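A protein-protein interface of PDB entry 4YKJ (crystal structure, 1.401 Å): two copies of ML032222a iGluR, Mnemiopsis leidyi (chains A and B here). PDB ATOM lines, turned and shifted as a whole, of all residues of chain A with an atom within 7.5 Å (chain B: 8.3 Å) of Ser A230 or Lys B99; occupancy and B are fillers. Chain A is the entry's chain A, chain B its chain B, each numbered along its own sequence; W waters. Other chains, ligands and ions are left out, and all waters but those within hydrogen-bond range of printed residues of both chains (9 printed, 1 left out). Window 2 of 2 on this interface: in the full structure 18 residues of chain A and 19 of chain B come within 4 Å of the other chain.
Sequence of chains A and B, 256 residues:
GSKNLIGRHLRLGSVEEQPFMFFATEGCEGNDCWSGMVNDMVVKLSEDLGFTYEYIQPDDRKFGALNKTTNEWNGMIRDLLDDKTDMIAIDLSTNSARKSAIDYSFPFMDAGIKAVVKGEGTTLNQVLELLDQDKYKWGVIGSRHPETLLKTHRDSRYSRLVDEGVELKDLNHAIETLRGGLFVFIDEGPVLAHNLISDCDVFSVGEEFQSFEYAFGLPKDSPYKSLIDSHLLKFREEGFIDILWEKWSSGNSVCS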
ATOM      1  N   LEU A  45      28.010   7.264 -24.920  1.00  0.00           N
ATOM      2  CA  LEU A  45      27.267   7.256 -26.189  1.00  0.00           C
ATOM      3  C   LEU A  45      27.031   5.834 -26.705  1.00  0.00           C
ATOM      4  O   LEU A  45      25.939   5.503 -27.144  1.00  0.00           O
ATOM      5  CB  LEU A  45      27.998   8.062 -27.256  1.00  0.00           C
ATOM      6  CG  LEU A  45      27.989   9.580 -27.063  1.00  0.00           C
ATOM      7  CD1 LEU A  45      28.993  10.219 -27.994  1.00  0.00           C
ATOM      8  CD2 LEU A  45      26.590  10.167 -27.281  1.00  0.00           C
ATOM      9  N   LEU A  49      23.336   4.438 -27.180  1.00  0.00           N
ATOM     10  CA  LEU A  49      22.901   4.342 -28.571  1.00  0.00           C
ATOM     11  C   LEU A  49      23.103   2.951 -29.187  1.00  0.00           C
ATOM     12  O   LEU A  49      22.557   2.659 -30.242  1.00  0.00           O
ATOM     13  CB  LEU A  49      23.586   5.421 -29.423  1.00  0.00           C
ATOM     14  CG  LEU A  49      23.158   6.849 -29.095  1.00  0.00           C
ATOM     15  CD1 LEU A  49      24.101   7.846 -29.654  1.00  0.00           C
ATOM     16  CD2 LEU A  49      21.754   7.107 -29.645  1.00  0.00           C
ATOM     17  N   PHE A 106      27.001  18.976 -32.195  1.00  0.00           N
ATOM     18  CA  PHE A 106      26.755  19.907 -31.111  1.00  0.00           C
ATOM     19  C   PHE A 106      28.037  20.045 -30.280  1.00  0.00           C
ATOM     20  O   PHE A 106      28.720  19.064 -30.032  1.00  0.00           O
ATOM     21  CB  PHE A 106      25.609  19.386 -30.248  1.00  0.00           C
ATOM     22  CG  PHE A 106      25.006  20.437 -29.396  1.00  0.00           C
ATOM     23  CD1 PHE A 106      24.091  21.329 -29.927  1.00  0.00           C
ATOM     24  CD2 PHE A 106      25.401  20.591 -28.084  1.00  0.00           C
ATOM     25  CE1 PHE A 106      23.543  22.344 -29.154  1.00  0.00           C
ATOM     26  CE2 PHE A 106      24.863  21.612 -27.302  1.00  0.00           C
ATOM     27  CZ  PHE A 106      23.940  22.489 -27.844  1.00  0.00           C
ATOM     28  N   TYR A 224      24.240   9.806 -38.840  1.00  0.00           N
ATOM     29  CA  TYR A 224      24.329   9.683 -37.389  1.00  0.00           C
ATOM     30  C   TYR A 224      24.346  11.034 -36.682  1.00  0.00           C
ATOM     31  O   TYR A 224      24.289  11.093 -35.453  1.00  0.00           O
ATOM     32  CB  TYR A 224      25.586   8.900 -37.014  1.00  0.00           C
ATOM     33  CG  TYR A 224      25.683   7.548 -37.687  1.00  0.00           C
ATOM     34  CD1 TYR A 224      24.586   6.702 -37.738  1.00  0.00           C
ATOM     35  CD2 TYR A 224      26.863   7.129 -38.272  1.00  0.00           C
ATOM     36  CE1 TYR A 224      24.656   5.461 -38.356  1.00  0.00           C
ATOM     37  CE2 TYR A 224      26.949   5.876 -38.895  1.00  0.00           C
ATOM     38  CZ  TYR A 224      25.833   5.060 -38.932  1.00  0.00           C
ATOM     39  OH  TYR A 224      25.895   3.819 -39.532  1.00  0.00           O
ATOM     40  N   LYS A 225      24.419  12.124 -37.438  1.00  0.00           N
ATOM     41  CA  LYS A 225      24.588  13.438 -36.812  1.00  0.00           C
ATOM     42  C   LYS A 225      23.456  13.800 -35.857  1.00  0.00           C
ATOM     43  O   LYS A 225      23.703  14.287 -34.758  1.00  0.00           O
ATOM     44  CB  LYS A 225      24.742  14.547 -37.856  1.00  0.00           C
ATOM     45  CG  LYS A 225      24.843  15.952 -37.244  1.00  0.00           C
ATOM     46  CD  LYS A 225      25.252  16.999 -38.263  1.00  0.00           C
ATOM     47  CE  LYS A 225      24.854  18.415 -37.821  1.00  0.00           C
ATOM     48  NZ  LYS A 225      25.436  18.872 -36.538  1.00  0.00           N
ATOM     49  N   SER A 226      22.225  13.567 -36.272  1.00  0.00           N
ATOM     50  CA  SER A 226      21.088  13.937 -35.441  1.00  0.00           C
ATOM     51  C   SER A 226      21.172  13.308 -34.057  1.00  0.00           C
ATOM     52  O   SER A 226      21.013  13.996 -33.031  1.00  0.00           O
ATOM     53  CB  SER A 226      19.792  13.500 -36.111  1.00  0.00           C
ATOM     54  OG  SER A 226      18.671  13.842 -35.313  1.00  0.00           O
ATOM     55  N   LEU A 227      21.412  12.002 -34.021  1.00  0.00           N
ATOM     56  CA  LEU A 227      21.466  11.278 -32.756  1.00  0.00           C
ATOM     57  C   LEU A 227      22.662  11.675 -31.910  1.00  0.00           C
ATOM     58  O   LEU A 227      22.549  11.863 -30.696  1.00  0.00           O
ATOM     59  CB  LEU A 227      21.477   9.764 -32.983  1.00  0.00           C
ATOM     60  CG  LEU A 227      20.109   9.126 -33.214  1.00  0.00           C
ATOM     61  CD1 LEU A 227      20.294   7.660 -33.607  1.00  0.00           C
ATOM     62  CD2 LEU A 227      19.246   9.237 -31.972  1.00  0.00           C
ATOM     63  N   ILE A 228      23.826  11.796 -32.529  1.00  0.00           N
ATOM     64  CA  ILE A 228      24.994  12.230 -31.778  1.00  0.00           C
ATOM     65  C   ILE A 228      24.742  13.631 -31.194  1.00  0.00           C
ATOM     66  O   ILE A 228      24.993  13.873 -30.015  1.00  0.00           O
ATOM     67  CB  ILE A 228      26.277  12.212 -32.650  1.00  0.00           C
ATOM     68  CG1 ILE A 228      26.665  10.774 -33.052  1.00  0.00           C
ATOM     69  CG2 ILE A 228      27.441  12.867 -31.918  1.00  0.00           C
ATOM     70  CD1 ILE A 228      27.016   9.833 -31.911  1.00  0.00           C
ATOM     71  N   ASP A 229      24.195  14.534 -31.997  1.00  0.00           N
ATOM     72  CA  ASP A 229      23.918  15.892 -31.512  1.00  0.00           C
ATOM     73  C   ASP A 229      22.962  15.896 -30.324  1.00  0.00           C
ATOM     74  O   ASP A 229      23.201  16.587 -29.328  1.00  0.00           O
ATOM     75  CB  ASP A 229      23.278  16.744 -32.611  1.00  0.00           C
ATOM     76  CG  ASP A 229      24.253  17.222 -33.650  1.00  0.00           C
ATOM     77  OD1 ASP A 229      25.459  16.984 -33.488  1.00  0.00           O
ATOM     78  OD2 ASP A 229      23.791  17.850 -34.626  1.00  0.00           O
ATOM     79  N   SER A 230      21.863  15.159 -30.443  1.00  0.00           N
ATOM     80  CA  SER A 230      20.869  15.108 -29.382  1.00  0.00           C
ATOM     81  C   SER A 230      21.490  14.624 -28.077  1.00  0.00           C
ATOM     82  O   SER A 230      21.270  15.200 -27.009  1.00  0.00           O
ATOM     83  CB  SER A 230      19.706  14.202 -29.788  1.00  0.00           C
ATOM     84  OG  SER A 230      18.907  14.827 -30.774  1.00  0.00           O
ATOM     85  N   HIS A 231      22.311  13.589 -28.173  1.00  0.00           N
ATOM     86  CA  HIS A 231      22.885  12.980 -26.988  1.00  0.00           C
ATOM     87  C   HIS A 231      23.972  13.861 -26.386  1.00  0.00           C
ATOM     88  O   HIS A 231      24.077  13.967 -25.173  1.00  0.00           O
ATOM     89  CB  HIS A 231      23.350  11.548 -27.280  1.00  0.00           C
ATOM     90  CG  HIS A 231      22.209  10.587 -27.333  1.00  0.00           C
ATOM     91  ND1 HIS A 231      22.014   9.599 -26.387  1.00  0.00           N
ATOM     92  CD2 HIS A 231      21.149  10.509 -28.171  1.00  0.00           C
ATOM     93  CE1 HIS A 231      20.911   8.930 -26.668  1.00  0.00           C
ATOM     94  NE2 HIS A 231      20.362   9.465 -27.749  1.00  0.00           N
ATOM     95  N   LEU A 232      24.750  14.534 -27.228  1.00  0.00           N
ATOM     96  CA  LEU A 232      25.727  15.482 -26.716  1.00  0.00           C
ATOM     97  C   LEU A 232      25.067  16.668 -26.017  1.00  0.00           C
ATOM     98  O   LEU A 232      25.543  17.124 -24.984  1.00  0.00           O
ATOM     99  CB  LEU A 232      26.661  15.958 -27.812  1.00  0.00           C
ATOM    100  CG  LEU A 232      27.670  14.910 -28.286  1.00  0.00           C
ATOM    101  CD1 LEU A 232      28.444  15.437 -29.482  1.00  0.00           C
ATOM    102  CD2 LEU A 232      28.606  14.471 -27.189  1.00  0.00           C
ATOM    103  N   LEU A 233      23.991  17.199 -26.581  1.00  0.00           N
ATOM    104  CA  LEU A 233      23.251  18.268 -25.908  1.00  0.00           C
ATOM    105  C   LEU A 233      22.769  17.800 -24.528  1.00  0.00           C
ATOM    106  O   LEU A 233      22.929  18.504 -23.533  1.00  0.00           O
ATOM    107  CB  LEU A 233      22.083  18.735 -26.784  1.00  0.00           C
ATOM    108  CG  LEU A 233      21.096  19.717 -26.138  1.00  0.00           C
ATOM    109  CD1 LEU A 233      21.777  20.960 -25.636  1.00  0.00           C
ATOM    110  CD2 LEU A 233      20.014  20.097 -27.138  1.00  0.00           C
ATOM    111  N   LYS A 234      22.194  16.600 -24.467  1.00  0.00           N
ATOM    112  CA  LYS A 234      21.738  16.046 -23.196  1.00  0.00           C
ATOM    113  C   LYS A 234      22.890  15.930 -22.196  1.00  0.00           C
ATOM    114  O   LYS A 234      22.735  16.259 -21.027  1.00  0.00           O
ATOM    115  CB  LYS A 234      21.092  14.683 -23.436  1.00  0.00           C
ATOM    116  CG  LYS A 234      20.439  14.048 -22.212  1.00  0.00           C
ATOM    117  CD  LYS A 234      19.677  12.786 -22.635  1.00  0.00           C
ATOM    118  CE  LYS A 234      19.201  11.942 -21.456  1.00  0.00           C
ATOM    119  NZ  LYS A 234      18.619  10.646 -21.904  1.00  0.00           N
ATOM    120  N   PHE A 235      24.047  15.471 -22.647  1.00  0.00           N
ATOM    121  CA  PHE A 235      25.225  15.413 -21.770  1.00  0.00           C
ATOM    122  C   PHE A 235      25.511  16.793 -21.166  1.00  0.00           C
ATOM    123  O   PHE A 235      25.812  16.910 -19.968  1.00  0.00           O
ATOM    124  CB  PHE A 235      26.502  15.002 -22.509  1.00  0.00           C
ATOM    125  CG  PHE A 235      26.599  13.543 -22.865  1.00  0.00           C
ATOM    126  CD1 PHE A 235      25.671  12.606 -22.459  1.00  0.00           C
ATOM    127  CD2 PHE A 235      27.671  13.114 -23.632  1.00  0.00           C
ATOM    128  CE1 PHE A 235      25.821  11.253 -22.817  1.00  0.00           C
ATOM    129  CE2 PHE A 235      27.821  11.786 -23.979  1.00  0.00           C
ATOM    130  CZ  PHE A 235      26.908  10.857 -23.587  1.00  0.00           C
ATOM    131  N   ARG A 236      25.435  17.836 -21.978  1.00  0.00           N
ATOM    132  CA  ARG A 236      25.753  19.146 -21.467  1.00  0.00           C
ATOM    133  C   ARG A 236      24.667  19.608 -20.502  1.00  0.00           C
ATOM    134  O   ARG A 236      24.966  20.083 -19.401  1.00  0.00           O
ATOM    135  CB  ARG A 236      25.937  20.133 -22.601  1.00  0.00           C
ATOM    136  CG  ARG A 236      26.707  21.348 -22.178  1.00  0.00           C
ATOM    137  CD  ARG A 236      27.314  22.031 -23.374  1.00  0.00           C
ATOM    138  NE  ARG A 236      28.305  23.016 -22.963  1.00  0.00           N
ATOM    139  CZ  ARG A 236      29.009  23.758 -23.810  1.00  0.00           C
ATOM    140  NH1 ARG A 236      28.834  23.614 -25.116  1.00  0.00           N
ATOM    141  NH2 ARG A 236      29.886  24.641 -23.351  1.00  0.00           N
ATOM    142  N   GLU A 237      23.414  19.421 -20.894  1.00  0.00           N
ATOM    143  CA  GLU A 237      22.279  19.870 -20.084  1.00  0.00           C
ATOM    144  C   GLU A 237      22.220  19.172 -18.719  1.00  0.00           C
ATOM    145  O   GLU A 237      21.877  19.803 -17.711  1.00  0.00           O
ATOM    146  CB  GLU A 237      20.991  19.668 -20.891  1.00  0.00           C
ATOM    147  CG  GLU A 237      19.757  20.212 -20.244  1.00  0.00           C
ATOM    148  CD  GLU A 237      18.563  20.161 -21.184  1.00  0.00           C
ATOM    149  OE1 GLU A 237      18.583  20.853 -22.224  1.00  0.00           O
ATOM    150  OE2 GLU A 237      17.591  19.440 -20.895  1.00  0.00           O
ATOM    151  N   TRP B  73       3.296  21.714 -28.895  1.00  0.00           N
ATOM    152  CA  TRP B  73       4.158  22.871 -28.734  1.00  0.00           C
ATOM    153  C   TRP B  73       3.354  24.152 -28.848  1.00  0.00           C
ATOM    154  O   TRP B  73       2.226  24.165 -29.329  1.00  0.00           O
ATOM    155  CB  TRP B  73       5.252  22.855 -29.807  1.00  0.00           C
ATOM    156  CG  TRP B  73       6.294  21.826 -29.543  1.00  0.00           C
ATOM    157  CD1 TRP B  73       6.315  20.528 -29.985  1.00  0.00           C
ATOM    158  CD2 TRP B  73       7.460  22.002 -28.743  1.00  0.00           C
ATOM    159  NE1 TRP B  73       7.443  19.896 -29.508  1.00  0.00           N
ATOM    160  CE2 TRP B  73       8.156  20.777 -28.736  1.00  0.00           C
ATOM    161  CE3 TRP B  73       7.985  23.080 -28.035  1.00  0.00           C
ATOM    162  CZ2 TRP B  73       9.362  20.612 -28.047  1.00  0.00           C
ATOM    163  CZ3 TRP B  73       9.164  22.921 -27.363  1.00  0.00           C
ATOM    164  CH2 TRP B  73       9.837  21.686 -27.356  1.00  0.00           C
ATOM    165  N   ILE B  77       8.277  27.966 -31.566  1.00  0.00           N
ATOM    166  CA  ILE B  77       8.580  26.586 -31.921  1.00  0.00           C
ATOM    167  C   ILE B  77       7.391  25.995 -32.684  1.00  0.00           C
ATOM    168  O   ILE B  77       7.562  25.368 -33.740  1.00  0.00           O
ATOM    169  CB  ILE B  77       8.886  25.727 -30.679  1.00  0.00           C
ATOM    170  CG1 ILE B  77      10.093  26.270 -29.883  1.00  0.00           C
ATOM    171  CG2 ILE B  77       9.082  24.286 -31.065  1.00  0.00           C
ATOM    172  CD1 ILE B  77      11.447  26.100 -30.532  1.00  0.00           C
ATOM    173  N   SER B  93      17.341  29.581 -26.937  1.00  0.00           N
ATOM    174  CA  SER B  93      18.190  28.713 -26.135  1.00  0.00           C
ATOM    175  C   SER B  93      18.099  27.262 -26.554  1.00  0.00           C
ATOM    176  O   SER B  93      17.027  26.771 -26.896  1.00  0.00           O
ATOM    177  CB  SER B  93      17.774  28.783 -24.676  1.00  0.00           C
ATOM    178  OG  SER B  93      17.876  30.119 -24.226  1.00  0.00           O
ATOM    179  N   THR B  94      19.232  26.592 -26.473  1.00  0.00           N
ATOM    180  CA  THR B  94      19.341  25.153 -26.711  1.00  0.00           C
ATOM    181  C   THR B  94      18.865  24.352 -25.502  1.00  0.00           C
ATOM    182  O   THR B  94      19.365  24.528 -24.386  1.00  0.00           O
ATOM    183  CB  THR B  94      20.789  24.757 -27.080  1.00  0.00           C
ATOM    184  OG1 THR B  94      21.688  25.225 -26.054  1.00  0.00           O
ATOM    185  CG2 THR B  94      21.180  25.342 -28.436  1.00  0.00           C
ATOM    186  N   ASN B  95      17.879  23.483 -25.721  1.00  0.00           N
ATOM    187  CA  ASN B  95      17.476  22.522 -24.712  1.00  0.00           C
ATOM    188  C   ASN B  95      17.021  21.242 -25.366  1.00  0.00           C
ATOM    189  O   ASN B  95      16.670  21.215 -26.553  1.00  0.00           O
ATOM    190  CB  ASN B  95      16.489  23.103 -23.671  1.00  0.00           C
ATOM    191  CG  ASN B  95      15.097  23.412 -24.215  1.00  0.00           C
ATOM    192  OD1 ASN B  95      14.440  22.573 -24.838  1.00  0.00           O
ATOM    193  ND2 ASN B  95      14.615  24.602 -23.911  1.00  0.00           N
ATOM    194  N   SER B  96      17.057  20.157 -24.590  1.00  0.00           N
ATOM    195  CA  SER B  96      16.759  18.843 -25.114  1.00  0.00           C
ATOM    196  C   SER B  96      15.311  18.707 -25.575  1.00  0.00           C
ATOM    197  O   SER B  96      15.043  18.053 -26.571  1.00  0.00           O
ATOM    198  CB  SER B  96      17.091  17.772 -24.074  1.00  0.00           C
ATOM    199  OG  SER B  96      18.493  17.644 -23.919  1.00  0.00           O
ATOM    200  N   ALA B  97      14.375  19.337 -24.875  1.00  0.00           N
ATOM    201  CA  ALA B  97      12.982  19.233 -25.299  1.00  0.00           C
ATOM    202  C   ALA B  97      12.817  19.770 -26.721  1.00  0.00           C
ATOM    203  O   ALA B  97      12.257  19.134 -27.610  1.00  0.00           O
ATOM    204  CB  ALA B  97      12.061  19.965 -24.332  1.00  0.00           C
ATOM    205  N   ARG B  98      13.339  20.965 -26.966  1.00  0.00           N
ATOM    206  CA  ARG B  98      13.259  21.543 -28.302  1.00  0.00           C
ATOM    207  C   ARG B  98      14.016  20.723 -29.331  1.00  0.00           C
ATOM    208  O   ARG B  98      13.555  20.568 -30.449  1.00  0.00           O
ATOM    209  CB  ARG B  98      13.789  22.964 -28.276  1.00  0.00           C
ATOM    210  CG  ARG B  98      12.858  23.944 -27.581  1.00  0.00           C
ATOM    211  CD  ARG B  98      13.535  25.268 -27.337  1.00  0.00           C
ATOM    212  NE  ARG B  98      12.610  26.225 -26.734  1.00  0.00           N
ATOM    213  CZ  ARG B  98      12.963  27.416 -26.273  1.00  0.00           C
ATOM    214  NH1 ARG B  98      14.235  27.815 -26.355  1.00  0.00           N
ATOM    215  NH2 ARG B  98      12.044  28.229 -25.764  1.00  0.00           N
ATOM    216  N   LYS B  99      15.175  20.194 -28.944  1.00  0.00           N
ATOM    217  CA  LYS B  99      15.996  19.398 -29.846  1.00  0.00           C
ATOM    218  C   LYS B  99      15.268  18.140 -30.309  1.00  0.00           C
ATOM    219  O   LYS B  99      15.586  17.599 -31.364  1.00  0.00           O
ATOM    220  CB  LYS B  99      17.325  19.044 -29.162  1.00  0.00           C
ATOM    221  CG  LYS B  99      18.315  18.216 -29.986  1.00  0.00           C
ATOM    222  CD  LYS B  99      18.819  18.955 -31.211  1.00  0.00           C
ATOM    223  CE  LYS B  99      19.857  18.139 -31.973  1.00  0.00           C
ATOM    224  NZ  LYS B  99      19.300  16.910 -32.600  1.00  0.00           N
ATOM    225  N   SER B 100      14.292  17.665 -29.535  1.00  0.00           N
ATOM    226  CA  SER B 100      13.523  16.505 -29.975  1.00  0.00           C
ATOM    227  C   SER B 100      12.650  16.851 -31.174  1.00  0.00           C
ATOM    228  O   SER B 100      12.341  15.977 -31.983  1.00  0.00           O
ATOM    229  CB  SER B 100      12.676  15.918 -28.836  1.00  0.00           C
ATOM    230  OG  SER B 100      11.582  16.749 -28.468  1.00  0.00           O
ATOM    231  N   ALA B 101      12.276  18.124 -31.289  1.00  0.00           N
ATOM    232  CA  ALA B 101      11.346  18.563 -32.336  1.00  0.00           C
ATOM    233  C   ALA B 101      11.962  19.360 -33.484  1.00  0.00           C
ATOM    234  O   ALA B 101      11.445  19.291 -34.595  1.00  0.00           O
ATOM    235  CB  ALA B 101      10.249  19.368 -31.709  1.00  0.00           C
ATOM    236  N   ILE B 102      13.007  20.146 -33.211  1.00  0.00           N
ATOM    237  CA  ILE B 102      13.631  21.011 -34.192  1.00  0.00           C
ATOM    238  C   ILE B 102      15.147  20.862 -34.131  1.00  0.00           C
ATOM    239  O   ILE B 102      15.692  20.220 -33.236  1.00  0.00           O
ATOM    240  CB  ILE B 102      13.258  22.525 -33.953  1.00  0.00           C
ATOM    241  CG1 ILE B 102      13.834  23.046 -32.629  1.00  0.00           C
ATOM    242  CG2 ILE B 102      11.762  22.737 -33.982  1.00  0.00           C
ATOM    243  CD1 ILE B 102      13.978  24.574 -32.594  1.00  0.00           C
ATOM    244  N   ASP B 103      15.818  21.464 -35.100  1.00  0.00           N
ATOM    245  CA  ASP B 103      17.262  21.581 -35.094  1.00  0.00           C
ATOM    246  C   ASP B 103      17.640  23.012 -34.706  1.00  0.00           C
ATOM    247  O   ASP B 103      16.805  23.932 -34.693  1.00  0.00           O
ATOM    248  CB  ASP B 103      17.839  21.270 -36.472  1.00  0.00           C
ATOM    249  CG  ASP B 103      17.889  19.795 -36.793  1.00  0.00           C
ATOM    250  OD1 ASP B 103      17.703  18.971 -35.877  1.00  0.00           O
ATOM    251  OD2 ASP B 103      18.160  19.471 -37.983  1.00  0.00           O
ATOM    252  N   TYR B 104      18.918  23.175 -34.405  1.00  0.00           N
ATOM    253  CA  TYR B 104      19.514  24.465 -34.131  1.00  0.00           C
ATOM    254  C   TYR B 104      20.601  24.773 -35.118  1.00  0.00           C
ATOM    255  O   TYR B 104      21.303  23.874 -35.593  1.00  0.00           O
ATOM    256  CB  TYR B 104      20.122  24.456 -32.746  1.00  0.00           C
ATOM    257  CG  TYR B 104      19.122  24.467 -31.611  1.00  0.00           C
ATOM    258  CD1 TYR B 104      18.560  25.660 -31.170  1.00  0.00           C
ATOM    259  CD2 TYR B 104      18.783  23.301 -30.961  1.00  0.00           C
ATOM    260  CE1 TYR B 104      17.696  25.695 -30.109  1.00  0.00           C
ATOM    261  CE2 TYR B 104      17.879  23.305 -29.896  1.00  0.00           C
ATOM    262  CZ  TYR B 104      17.346  24.514 -29.479  1.00  0.00           C
ATOM    263  OH  TYR B 104      16.510  24.535 -28.378  1.00  0.00           O
ATOM    264  N   LEU B 218      15.797  25.833 -36.566  1.00  0.00           N
ATOM    265  CA  LEU B 218      15.569  25.389 -37.926  1.00  0.00           C
ATOM    266  C   LEU B 218      14.721  24.116 -37.899  1.00  0.00           C
ATOM    267  O   LEU B 218      14.863  23.280 -37.009  1.00  0.00           O
ATOM    268  CB  LEU B 218      16.913  25.111 -38.604  1.00  0.00           C
ATOM    269  CG  LEU B 218      17.729  26.365 -38.925  1.00  0.00           C
ATOM    270  CD1 LEU B 218      19.187  25.978 -39.137  1.00  0.00           C
ATOM    271  CD2 LEU B 218      17.152  26.992 -40.166  1.00  0.00           C
ATOM    272  N   LYS B 220      13.712  20.336 -38.806  1.00  0.00           N
ATOM    273  CA  LYS B 220      14.472  19.175 -39.226  1.00  0.00           C
ATOM    274  C   LYS B 220      14.417  19.069 -40.750  1.00  0.00           C
ATOM    275  O   LYS B 220      13.398  19.404 -41.391  1.00  0.00           O
ATOM    276  CB  LYS B 220      13.938  17.911 -38.550  1.00  0.00           C
ATOM    277  CG  LYS B 220      14.193  17.902 -37.044  1.00  0.00           C
ATOM    278  CD  LYS B 220      13.659  16.662 -36.386  1.00  0.00           C
ATOM    279  CE  LYS B 220      14.116  16.606 -34.966  1.00  0.00           C
ATOM    280  NZ  LYS B 220      14.036  15.222 -34.413  1.00  0.00           N
ATOM    281  N   LYS B 225      20.066  24.751 -43.618  1.00  0.00           N
ATOM    282  CA  LYS B 225      20.852  24.693 -42.389  1.00  0.00           C
ATOM    283  C   LYS B 225      22.355  24.803 -42.647  1.00  0.00           C
ATOM    284  O   LYS B 225      23.046  25.528 -41.940  1.00  0.00           O
ATOM    285  CB  LYS B 225      20.534  23.419 -41.607  1.00  0.00           C
ATOM    286  CG  LYS B 225      21.407  23.263 -40.368  1.00  0.00           C
ATOM    287  CD  LYS B 225      20.944  22.136 -39.463  1.00  0.00           C
ATOM    288  CE  LYS B 225      22.072  21.625 -38.563  1.00  0.00           C
ATOM    289  NZ  LYS B 225      22.653  22.676 -37.693  1.00  0.00           N
HETATM  290  O   HOH W   1      18.956  16.713 -26.526  1.00  0.00           O
HETATM  291  O   HOH W   2      21.123  17.988 -35.097  1.00  0.00           O
HETATM  292  O   HOH W   3      15.850  15.012 -32.449  1.00  0.00           O
HETATM  293  O   HOH W   4      17.668  16.270 -36.262  1.00  0.00           O
HETATM  294  O   HOH W   5      20.355  22.947 -22.352  1.00  0.00           O
HETATM  295  O   HOH W   6      25.735  21.693 -36.595  1.00  0.00           O
HETATM  296  O   HOH W   7      23.659  21.491 -35.174  1.00  0.00           O
HETATM  297  O   HOH W   8      14.958  20.172 -21.865  1.00  0.00           O
HETATM  298  O   HOH W   9      15.561  13.252 -36.228  1.00  0.00           O
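OG of Ser A230 lies within hydrogen-bond range of NZ of Lys B99, 2.8 Å away.
The side-chain carboxylate of Glu A237 sits at hydrogen-bond distance from the backbone NH of Ser B96 (2.9 Å).
The backbone carbonyl oxygen (O) of Ser A226 lies within hydrogen-bond range of the side-chain amino group (NZ) of Lys B99 (3.4 Å).
The backbone NH (N) of Arg B98 lies within hydrogen-bond range of the side-chain amide oxygen (OD1) of Asn B95, 2.9 Å away.
The backbone NH (N) of Asn B95 lies within hydrogen-bond range of the side-chain hydroxyl (OH) of Tyr B104 (3.2 Å).
O of Ser A226 sits at hydrogen-bond distance from OG of Ser A230, at 3.2 Å.
The backbone NH (N) of Ala B97 sits at hydrogen-bond distance from the side-chain amide oxygen (OD1) of Asn B95, 3.2 Å away.
OD1 of Asp A229 sits at hydrogen-bond distance from N of Phe A106, at 2.8 Å.
The side-chain amino group (NZ) of Lys A225 lies within salt-bridge range of the side-chain carboxylate (OD2) of Asp A229 (2.7 Å).
CE1 of Phe A106 touches CG2 of Thr B94 (3.9 Å).
Asp A229 touches Lys B99.
Asn B95 touches Leu A233.
Ser B96 touches Leu A233.
Leu A233 touches Lys B99.
Ser B96 touches Lys A234 (OG to CA, 3.7 Å).
CA of Asn B95 touches OE1 of Glu A237 (3.2 Å).
Of the printed residues of chain B, Ser A230 touches Lys B99 (2.8 Å).
Of the printed residues of chain A, Lys B99 touches Ser A226, Asp A229, Ser A230 and Leu A233.
Printed residues of chain B within 4 Å of Phe A106: Thr B94.
Printed residues of chain A within 4 Å of Ser B96: Leu A233, Lys A234 and Glu A237.
Printed residues of chain B within 4 Å of Asp A229: Lys B99.
Phe A235 touches none of the printed residues of chain B.
Ala B97 touches none of the printed residues of chain A.
The nearest printed residue of chain B that does not touch Ser A230 is Ser B96 (4.8 Å).
The nearest printed residue of chain A that does not touch Lys B99 is Leu A227 (5.5 Å).
Of the 17 printed residues of chain B, 4 touch a printed residue of chain A.
Hydrophobic or aromatic side chains of chain A within 4 Å of the printed part of chain B: Phe A106 and Leu A233.
Among the printed residues, 10 pairs touch across the chains.
Among the printed residues, no Asp or Glu carboxylate lies within 4 Å of a Lys or Arg side-chain nitrogen of the other chain.
1 position is printed for both chains.
Water W3 lies within hydrogen-bond range of the side-chain amino group of Lys B220 (2.7 Å), the backbone carbonyl oxygen of Lys B99 (2.8 Å) and the side-chain hydroxyl of Ser A230 (3.5 Å).
Water W2 bridges OD2 of Asp A229 and NZ of Lys B99.
Water W4 lies within hydrogen-bond range of OD1 of Asp B103 (2.7 Å) and OG of Ser A226 (2.8 Å).
Water W5 lies within hydrogen-bond range of OE1 of Glu A237 and O of Thr B94.
Water W6 bridges the side-chain amino group (NZ) of Lys A225 (2.8 Å) and the side-chain amino group (NZ) of Lys B225 (3.4 Å).
Water W9 bridges NZ of Lys B220 (3.1 Å) and OG of Ser A226 (3.3 Å).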
